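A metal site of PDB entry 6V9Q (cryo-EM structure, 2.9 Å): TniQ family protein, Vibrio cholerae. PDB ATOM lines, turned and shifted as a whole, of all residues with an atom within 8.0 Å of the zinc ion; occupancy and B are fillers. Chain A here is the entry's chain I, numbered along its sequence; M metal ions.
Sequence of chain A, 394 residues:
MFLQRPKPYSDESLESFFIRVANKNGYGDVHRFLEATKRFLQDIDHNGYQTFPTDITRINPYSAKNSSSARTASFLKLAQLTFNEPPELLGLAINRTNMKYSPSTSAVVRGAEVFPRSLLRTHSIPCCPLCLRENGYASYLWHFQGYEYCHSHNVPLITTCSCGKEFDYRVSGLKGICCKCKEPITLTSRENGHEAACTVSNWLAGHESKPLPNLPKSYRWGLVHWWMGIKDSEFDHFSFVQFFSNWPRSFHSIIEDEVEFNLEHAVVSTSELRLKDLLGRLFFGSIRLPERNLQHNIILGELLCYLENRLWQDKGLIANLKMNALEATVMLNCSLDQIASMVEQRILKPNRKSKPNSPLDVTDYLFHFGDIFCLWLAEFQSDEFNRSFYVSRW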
ATOM      1  N   CYS A 127      16.734 -11.491   8.120  1.00  0.00           N
ATOM      2  CA  CYS A 127      17.355 -12.504   7.288  1.00  0.00           C
ATOM      3  C   CYS A 127      16.394 -12.915   6.182  1.00  0.00           C
ATOM      4  O   CYS A 127      15.202 -12.627   6.230  1.00  0.00           O
ATOM      5  CB  CYS A 127      17.761 -13.718   8.118  1.00  0.00           C
ATOM      6  SG  CYS A 127      16.358 -14.596   8.815  1.00  0.00           S
ATOM      7  N   CYS A 128      16.945 -13.596   5.185  1.00  0.00           N
ATOM      8  CA  CYS A 128      16.160 -14.211   4.121  1.00  0.00           C
ATOM      9  C   CYS A 128      16.357 -15.718   4.184  1.00  0.00           C
ATOM     10  O   CYS A 128      17.483 -16.206   3.947  1.00  0.00           O
ATOM     11  CB  CYS A 128      16.560 -13.677   2.752  1.00  0.00           C
ATOM     12  SG  CYS A 128      15.616 -14.388   1.381  1.00  0.00           S
ATOM     13  N   PRO A 129      15.318 -16.495   4.497  1.00  0.00           N
ATOM     14  CA  PRO A 129      15.508 -17.953   4.632  1.00  0.00           C
ATOM     15  C   PRO A 129      15.718 -18.679   3.311  1.00  0.00           C
ATOM     16  O   PRO A 129      16.145 -19.831   3.330  1.00  0.00           O
ATOM     17  CB  PRO A 129      14.198 -18.410   5.303  1.00  0.00           C
ATOM     18  CG  PRO A 129      13.203 -17.388   4.886  1.00  0.00           C
ATOM     19  CD  PRO A 129      13.941 -16.084   4.800  1.00  0.00           C
ATOM     20  N   LEU A 130      15.422 -18.041   2.180  1.00  0.00           N
ATOM     21  CA  LEU A 130      15.691 -18.675   0.895  1.00  0.00           C
ATOM     22  C   LEU A 130      17.183 -18.657   0.575  1.00  0.00           C
ATOM     23  O   LEU A 130      17.710 -19.606  -0.021  1.00  0.00           O
ATOM     24  CB  LEU A 130      14.902 -17.985  -0.222  1.00  0.00           C
ATOM     25  CG  LEU A 130      13.443 -18.383  -0.463  1.00  0.00           C
ATOM     26  CD1 LEU A 130      12.495 -17.825   0.590  1.00  0.00           C
ATOM     27  CD2 LEU A 130      13.011 -17.954  -1.864  1.00  0.00           C
ATOM     28  N   CYS A 131      17.880 -17.590   0.971  1.00  0.00           N
ATOM     29  CA  CYS A 131      19.320 -17.543   0.779  1.00  0.00           C
ATOM     30  C   CYS A 131      20.042 -18.458   1.756  1.00  0.00           C
ATOM     31  O   CYS A 131      21.132 -18.955   1.463  1.00  0.00           O
ATOM     32  CB  CYS A 131      19.834 -16.113   0.936  1.00  0.00           C
ATOM     33  SG  CYS A 131      19.249 -14.963  -0.326  1.00  0.00           S
ATOM     34  N   LEU A 132      19.439 -18.714   2.925  1.00  0.00           N
ATOM     35  CA  LEU A 132      20.045 -19.589   3.922  1.00  0.00           C
ATOM     36  C   LEU A 132      20.023 -21.046   3.498  1.00  0.00           C
ATOM     37  O   LEU A 132      20.869 -21.826   3.958  1.00  0.00           O
ATOM     38  CB  LEU A 132      19.333 -19.431   5.259  1.00  0.00           C
ATOM     39  CG  LEU A 132      19.453 -18.065   5.948  1.00  0.00           C
ATOM     40  CD1 LEU A 132      18.582 -18.013   7.194  1.00  0.00           C
ATOM     41  CD2 LEU A 132      20.905 -17.763   6.286  1.00  0.00           C
ATOM     42  N   GLU A 134      19.877 -21.985   0.067  1.00  0.00           N
ATOM     43  CA  GLU A 134      20.476 -22.116  -1.254  1.00  0.00           C
ATOM     44  C   GLU A 134      21.961 -21.761  -1.233  1.00  0.00           C
ATOM     45  O   GLU A 134      22.801 -22.554  -1.665  1.00  0.00           O
ATOM     46  CB  GLU A 134      19.733 -21.222  -2.251  1.00  0.00           C
ATOM     47  CG  GLU A 134      18.321 -21.684  -2.564  1.00  0.00           C
ATOM     48  CD  GLU A 134      17.613 -20.766  -3.543  1.00  0.00           C
ATOM     49  OE1 GLU A 134      18.184 -19.711  -3.879  1.00  0.00           O
ATOM     50  OE2 GLU A 134      16.498 -21.107  -3.985  1.00  0.00           O
ATOM     51  N   ASN A 135      22.301 -20.581  -0.715  1.00  0.00           N
ATOM     52  CA  ASN A 135      23.707 -20.188  -0.631  1.00  0.00           C
ATOM     53  C   ASN A 135      24.410 -20.883   0.534  1.00  0.00           C
ATOM     54  O   ASN A 135      25.586 -21.254   0.412  1.00  0.00           O
ATOM     55  CB  ASN A 135      23.805 -18.672  -0.481  1.00  0.00           C
ATOM     56  CG  ASN A 135      23.428 -17.937  -1.755  1.00  0.00           C
ATOM     57  OD1 ASN A 135      23.807 -18.342  -2.854  1.00  0.00           O
ATOM     58  ND2 ASN A 135      22.676 -16.852  -1.608  1.00  0.00           N
ATOM     59  N   SER A 139      24.593 -12.813   4.320  1.00  0.00           N
ATOM     60  CA  SER A 139      25.257 -11.686   3.699  1.00  0.00           C
ATOM     61  C   SER A 139      25.379 -10.515   4.683  1.00  0.00           C
ATOM     62  O   SER A 139      24.649 -10.425   5.670  1.00  0.00           O
ATOM     63  CB  SER A 139      24.506 -11.232   2.449  1.00  0.00           C
ATOM     64  OG  SER A 139      25.133 -10.105   1.866  1.00  0.00           O
ATOM     65  N   TRP A 142      22.400  -7.578   5.486  1.00  0.00           N
ATOM     66  CA  TRP A 142      21.333  -7.730   6.455  1.00  0.00           C
ATOM     67  C   TRP A 142      21.588  -6.952   7.735  1.00  0.00           C
ATOM     68  O   TRP A 142      20.680  -6.832   8.566  1.00  0.00           O
ATOM     69  CB  TRP A 142      21.141  -9.218   6.773  1.00  0.00           C
ATOM     70  CG  TRP A 142      20.707 -10.051   5.591  1.00  0.00           C
ATOM     71  CD1 TRP A 142      20.312  -9.594   4.364  1.00  0.00           C
ATOM     72  CD2 TRP A 142      20.638 -11.481   5.513  1.00  0.00           C
ATOM     73  NE1 TRP A 142      19.993 -10.653   3.543  1.00  0.00           N
ATOM     74  CE2 TRP A 142      20.189 -11.816   4.227  1.00  0.00           C
ATOM     75  CE3 TRP A 142      20.906 -12.511   6.423  1.00  0.00           C
ATOM     76  CZ2 TRP A 142      19.992 -13.133   3.821  1.00  0.00           C
ATOM     77  CZ3 TRP A 142      20.715 -13.820   6.019  1.00  0.00           C
ATOM     78  CH2 TRP A 142      20.264 -14.118   4.729  1.00  0.00           C
ATOM     79  N   TYR A 147      18.148  -1.746   3.376  1.00  0.00           N
ATOM     80  CA  TYR A 147      18.118  -3.002   2.628  1.00  0.00           C
ATOM     81  C   TYR A 147      16.980  -3.846   3.197  1.00  0.00           C
ATOM     82  O   TYR A 147      17.167  -4.618   4.139  1.00  0.00           O
ATOM     83  CB  TYR A 147      19.455  -3.718   2.713  1.00  0.00           C
ATOM     84  CG  TYR A 147      19.536  -4.958   1.853  1.00  0.00           C
ATOM     85  CD1 TYR A 147      19.762  -4.861   0.481  1.00  0.00           C
ATOM     86  CD2 TYR A 147      19.389  -6.222   2.399  1.00  0.00           C
ATOM     87  CE1 TYR A 147      19.841  -5.983  -0.316  1.00  0.00           C
ATOM     88  CE2 TYR A 147      19.465  -7.354   1.612  1.00  0.00           C
ATOM     89  CZ  TYR A 147      19.689  -7.233   0.265  1.00  0.00           C
ATOM     90  OH  TYR A 147      19.769  -8.355  -0.532  1.00  0.00           O
ATOM     91  N   TYR A 149      14.393  -5.614   1.110  1.00  0.00           N
ATOM     92  CA  TYR A 149      14.027  -6.775   0.311  1.00  0.00           C
ATOM     93  C   TYR A 149      15.292  -7.476  -0.178  1.00  0.00           C
ATOM     94  O   TYR A 149      16.380  -6.889  -0.213  1.00  0.00           O
ATOM     95  CB  TYR A 149      13.153  -6.397  -0.898  1.00  0.00           C
ATOM     96  CG  TYR A 149      11.758  -5.902  -0.587  1.00  0.00           C
ATOM     97  CD1 TYR A 149      11.225  -5.957   0.698  1.00  0.00           C
ATOM     98  CD2 TYR A 149      10.940  -5.402  -1.599  1.00  0.00           C
ATOM     99  CE1 TYR A 149       9.950  -5.504   0.968  1.00  0.00           C
ATOM    100  CE2 TYR A 149       9.664  -4.948  -1.339  1.00  0.00           C
ATOM    101  CZ  TYR A 149       9.177  -5.011  -0.044  1.00  0.00           C
ATOM    102  OH  TYR A 149       7.905  -4.572   0.223  1.00  0.00           O
ATOM    103  N   CYS A 150      15.132  -8.735  -0.549  1.00  0.00           N
ATOM    104  CA  CYS A 150      16.230  -9.463  -1.164  1.00  0.00           C
ATOM    105  C   CYS A 150      16.437  -9.002  -2.602  1.00  0.00           C
ATOM    106  O   CYS A 150      15.472  -8.850  -3.358  1.00  0.00           O
ATOM    107  CB  CYS A 150      15.960 -10.969  -1.134  1.00  0.00           C
ATOM    108  SG  CYS A 150      17.282 -11.961  -1.862  1.00  0.00           S
ATOM    109  N   HIS A 151      17.693  -8.776  -2.963  1.00  0.00           N
ATOM    110  CA  HIS A 151      18.007  -8.294  -4.304  1.00  0.00           C
ATOM    111  C   HIS A 151      18.036  -9.394  -5.346  1.00  0.00           C
ATOM    112  O   HIS A 151      18.215  -9.095  -6.538  1.00  0.00           O
ATOM    113  CB  HIS A 151      19.345  -7.552  -4.299  1.00  0.00           C
ATOM    114  CG  HIS A 151      20.524  -8.426  -3.995  1.00  0.00           C
ATOM    115  ND1 HIS A 151      20.879  -8.797  -2.724  1.00  0.00           N
ATOM    116  CD2 HIS A 151      21.430  -9.003  -4.825  1.00  0.00           C
ATOM    117  CE1 HIS A 151      21.945  -9.568  -2.761  1.00  0.00           C
ATOM    118  NE2 HIS A 151      22.306  -9.711  -4.027  1.00  0.00           N
ATOM    119  N   SER A 152      17.879 -10.657  -4.953  1.00  0.00           N
ATOM    120  CA  SER A 152      17.838 -11.763  -5.889  1.00  0.00           C
ATOM    121  C   SER A 152      16.608 -12.644  -5.775  1.00  0.00           C
ATOM    122  O   SER A 152      16.372 -13.466  -6.663  1.00  0.00           O
ATOM    123  CB  SER A 152      19.090 -12.643  -5.735  1.00  0.00           C
ATOM    124  OG  SER A 152      20.262 -11.928  -6.084  1.00  0.00           O
ATOM    125  N   HIS A 153      15.812 -12.501  -4.713  1.00  0.00           N
ATOM    126  CA  HIS A 153      14.580 -13.250  -4.564  1.00  0.00           C
ATOM    127  C   HIS A 153      13.333 -12.385  -4.474  1.00  0.00           C
ATOM    128  O   HIS A 153      12.223 -12.914  -4.589  1.00  0.00           O
ATOM    129  CB  HIS A 153      14.646 -14.161  -3.324  1.00  0.00           C
ATOM    130  CG  HIS A 153      15.676 -15.241  -3.420  1.00  0.00           C
ATOM    131  ND1 HIS A 153      16.969 -15.079  -2.983  1.00  0.00           N
ATOM    132  CD2 HIS A 153      15.602 -16.491  -3.931  1.00  0.00           C
ATOM    133  CE1 HIS A 153      17.643 -16.193  -3.202  1.00  0.00           C
ATOM    134  NE2 HIS A 153      16.845 -17.065  -3.771  1.00  0.00           N
ATOM    135  N   ASN A 154      13.495 -11.072  -4.249  1.00  0.00           N
ATOM    136  CA  ASN A 154      12.408 -10.071  -4.207  1.00  0.00           C
ATOM    137  C   ASN A 154      11.368 -10.404  -3.131  1.00  0.00           C
ATOM    138  O   ASN A 154      10.170 -10.185  -3.312  1.00  0.00           O
ATOM    139  CB  ASN A 154      11.747  -9.912  -5.580  1.00  0.00           C
ATOM    140  CG  ASN A 154      12.717  -9.414  -6.633  1.00  0.00           C
ATOM    141  OD1 ASN A 154      13.022 -10.112  -7.595  1.00  0.00           O
ATOM    142  ND2 ASN A 154      13.200  -8.192  -6.457  1.00  0.00           N
ATOM    143  N   VAL A 155      11.844 -10.934  -2.006  1.00  0.00           N
ATOM    144  CA  VAL A 155      10.980 -11.301  -0.888  1.00  0.00           C
ATOM    145  C   VAL A 155      11.368 -10.427   0.300  1.00  0.00           C
ATOM    146  O   VAL A 155      12.546 -10.103   0.469  1.00  0.00           O
ATOM    147  CB  VAL A 155      11.088 -12.819  -0.613  1.00  0.00           C
ATOM    148  CG1 VAL A 155      12.527 -13.230  -0.287  1.00  0.00           C
ATOM    149  CG2 VAL A 155      10.153 -13.271   0.493  1.00  0.00           C
ATOM    150  N   PRO A 156      10.403  -9.941   1.095  1.00  0.00           N
ATOM    151  CA  PRO A 156      10.771  -9.149   2.272  1.00  0.00           C
ATOM    152  C   PRO A 156      11.432  -9.980   3.349  1.00  0.00           C
ATOM    153  O   PRO A 156      11.157 -11.165   3.521  1.00  0.00           O
ATOM    154  CB  PRO A 156       9.425  -8.586   2.752  1.00  0.00           C
ATOM    155  CG  PRO A 156       8.389  -9.465   2.145  1.00  0.00           C
ATOM    156  CD  PRO A 156       8.954  -9.875   0.822  1.00  0.00           C
ATOM    157  N   LEU A 157      12.345  -9.326   4.073  1.00  0.00           N
ATOM    158  CA  LEU A 157      13.091  -9.984   5.143  1.00  0.00           C
ATOM    159  C   LEU A 157      12.189 -10.222   6.344  1.00  0.00           C
ATOM    160  O   LEU A 157      11.105  -9.638   6.476  1.00  0.00           O
ATOM    161  CB  LEU A 157      14.292  -9.133   5.547  1.00  0.00           C
ATOM    162  CG  LEU A 157      15.348  -8.872   4.476  1.00  0.00           C
ATOM    163  CD1 LEU A 157      16.426  -7.933   5.013  1.00  0.00           C
ATOM    164  CD2 LEU A 157      15.951 -10.164   3.970  1.00  0.00           C
HETATM  165 ZN    ZN M   1      17.445 -13.326   0.199  1.00  0.00          ZN
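The zinc ion is bound by the side-chain sulfur of Cys 128 (2.4 Å), the side-chain sulfur of Cys 150 (2.5 Å) and the side-chain sulfur of Cys 131 (2.5 Å).
ND1 of His 153 touches the zinc ion (3.7 Å). Within 4 Å of the zinc ion: Cys 128, Cys 131, Cys 150 and His 153. The nearest printed residue that does not touch the zinc ion is Trp 142 (4.4 Å).
SG of Cys 128 lies close to N of Leu 130 (3.7 Å). SG of Cys 150 lies close to N of His 153 (3.3 Å). O of Val 155 is in hydrogen-bond range of N of Cys 150, at 3.1 Å. SG of Cys 150 lies close to N of Ser 152, at 3.4 Å. A ring nitrogen (ND1) of His 153 lies close to the side-chain sulfur (SG) of Cys 131 (3.5 Å). NE2 of His 153 sits at hydrogen-bond distance from OE1 of Glu 134, at 3.0 Å.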
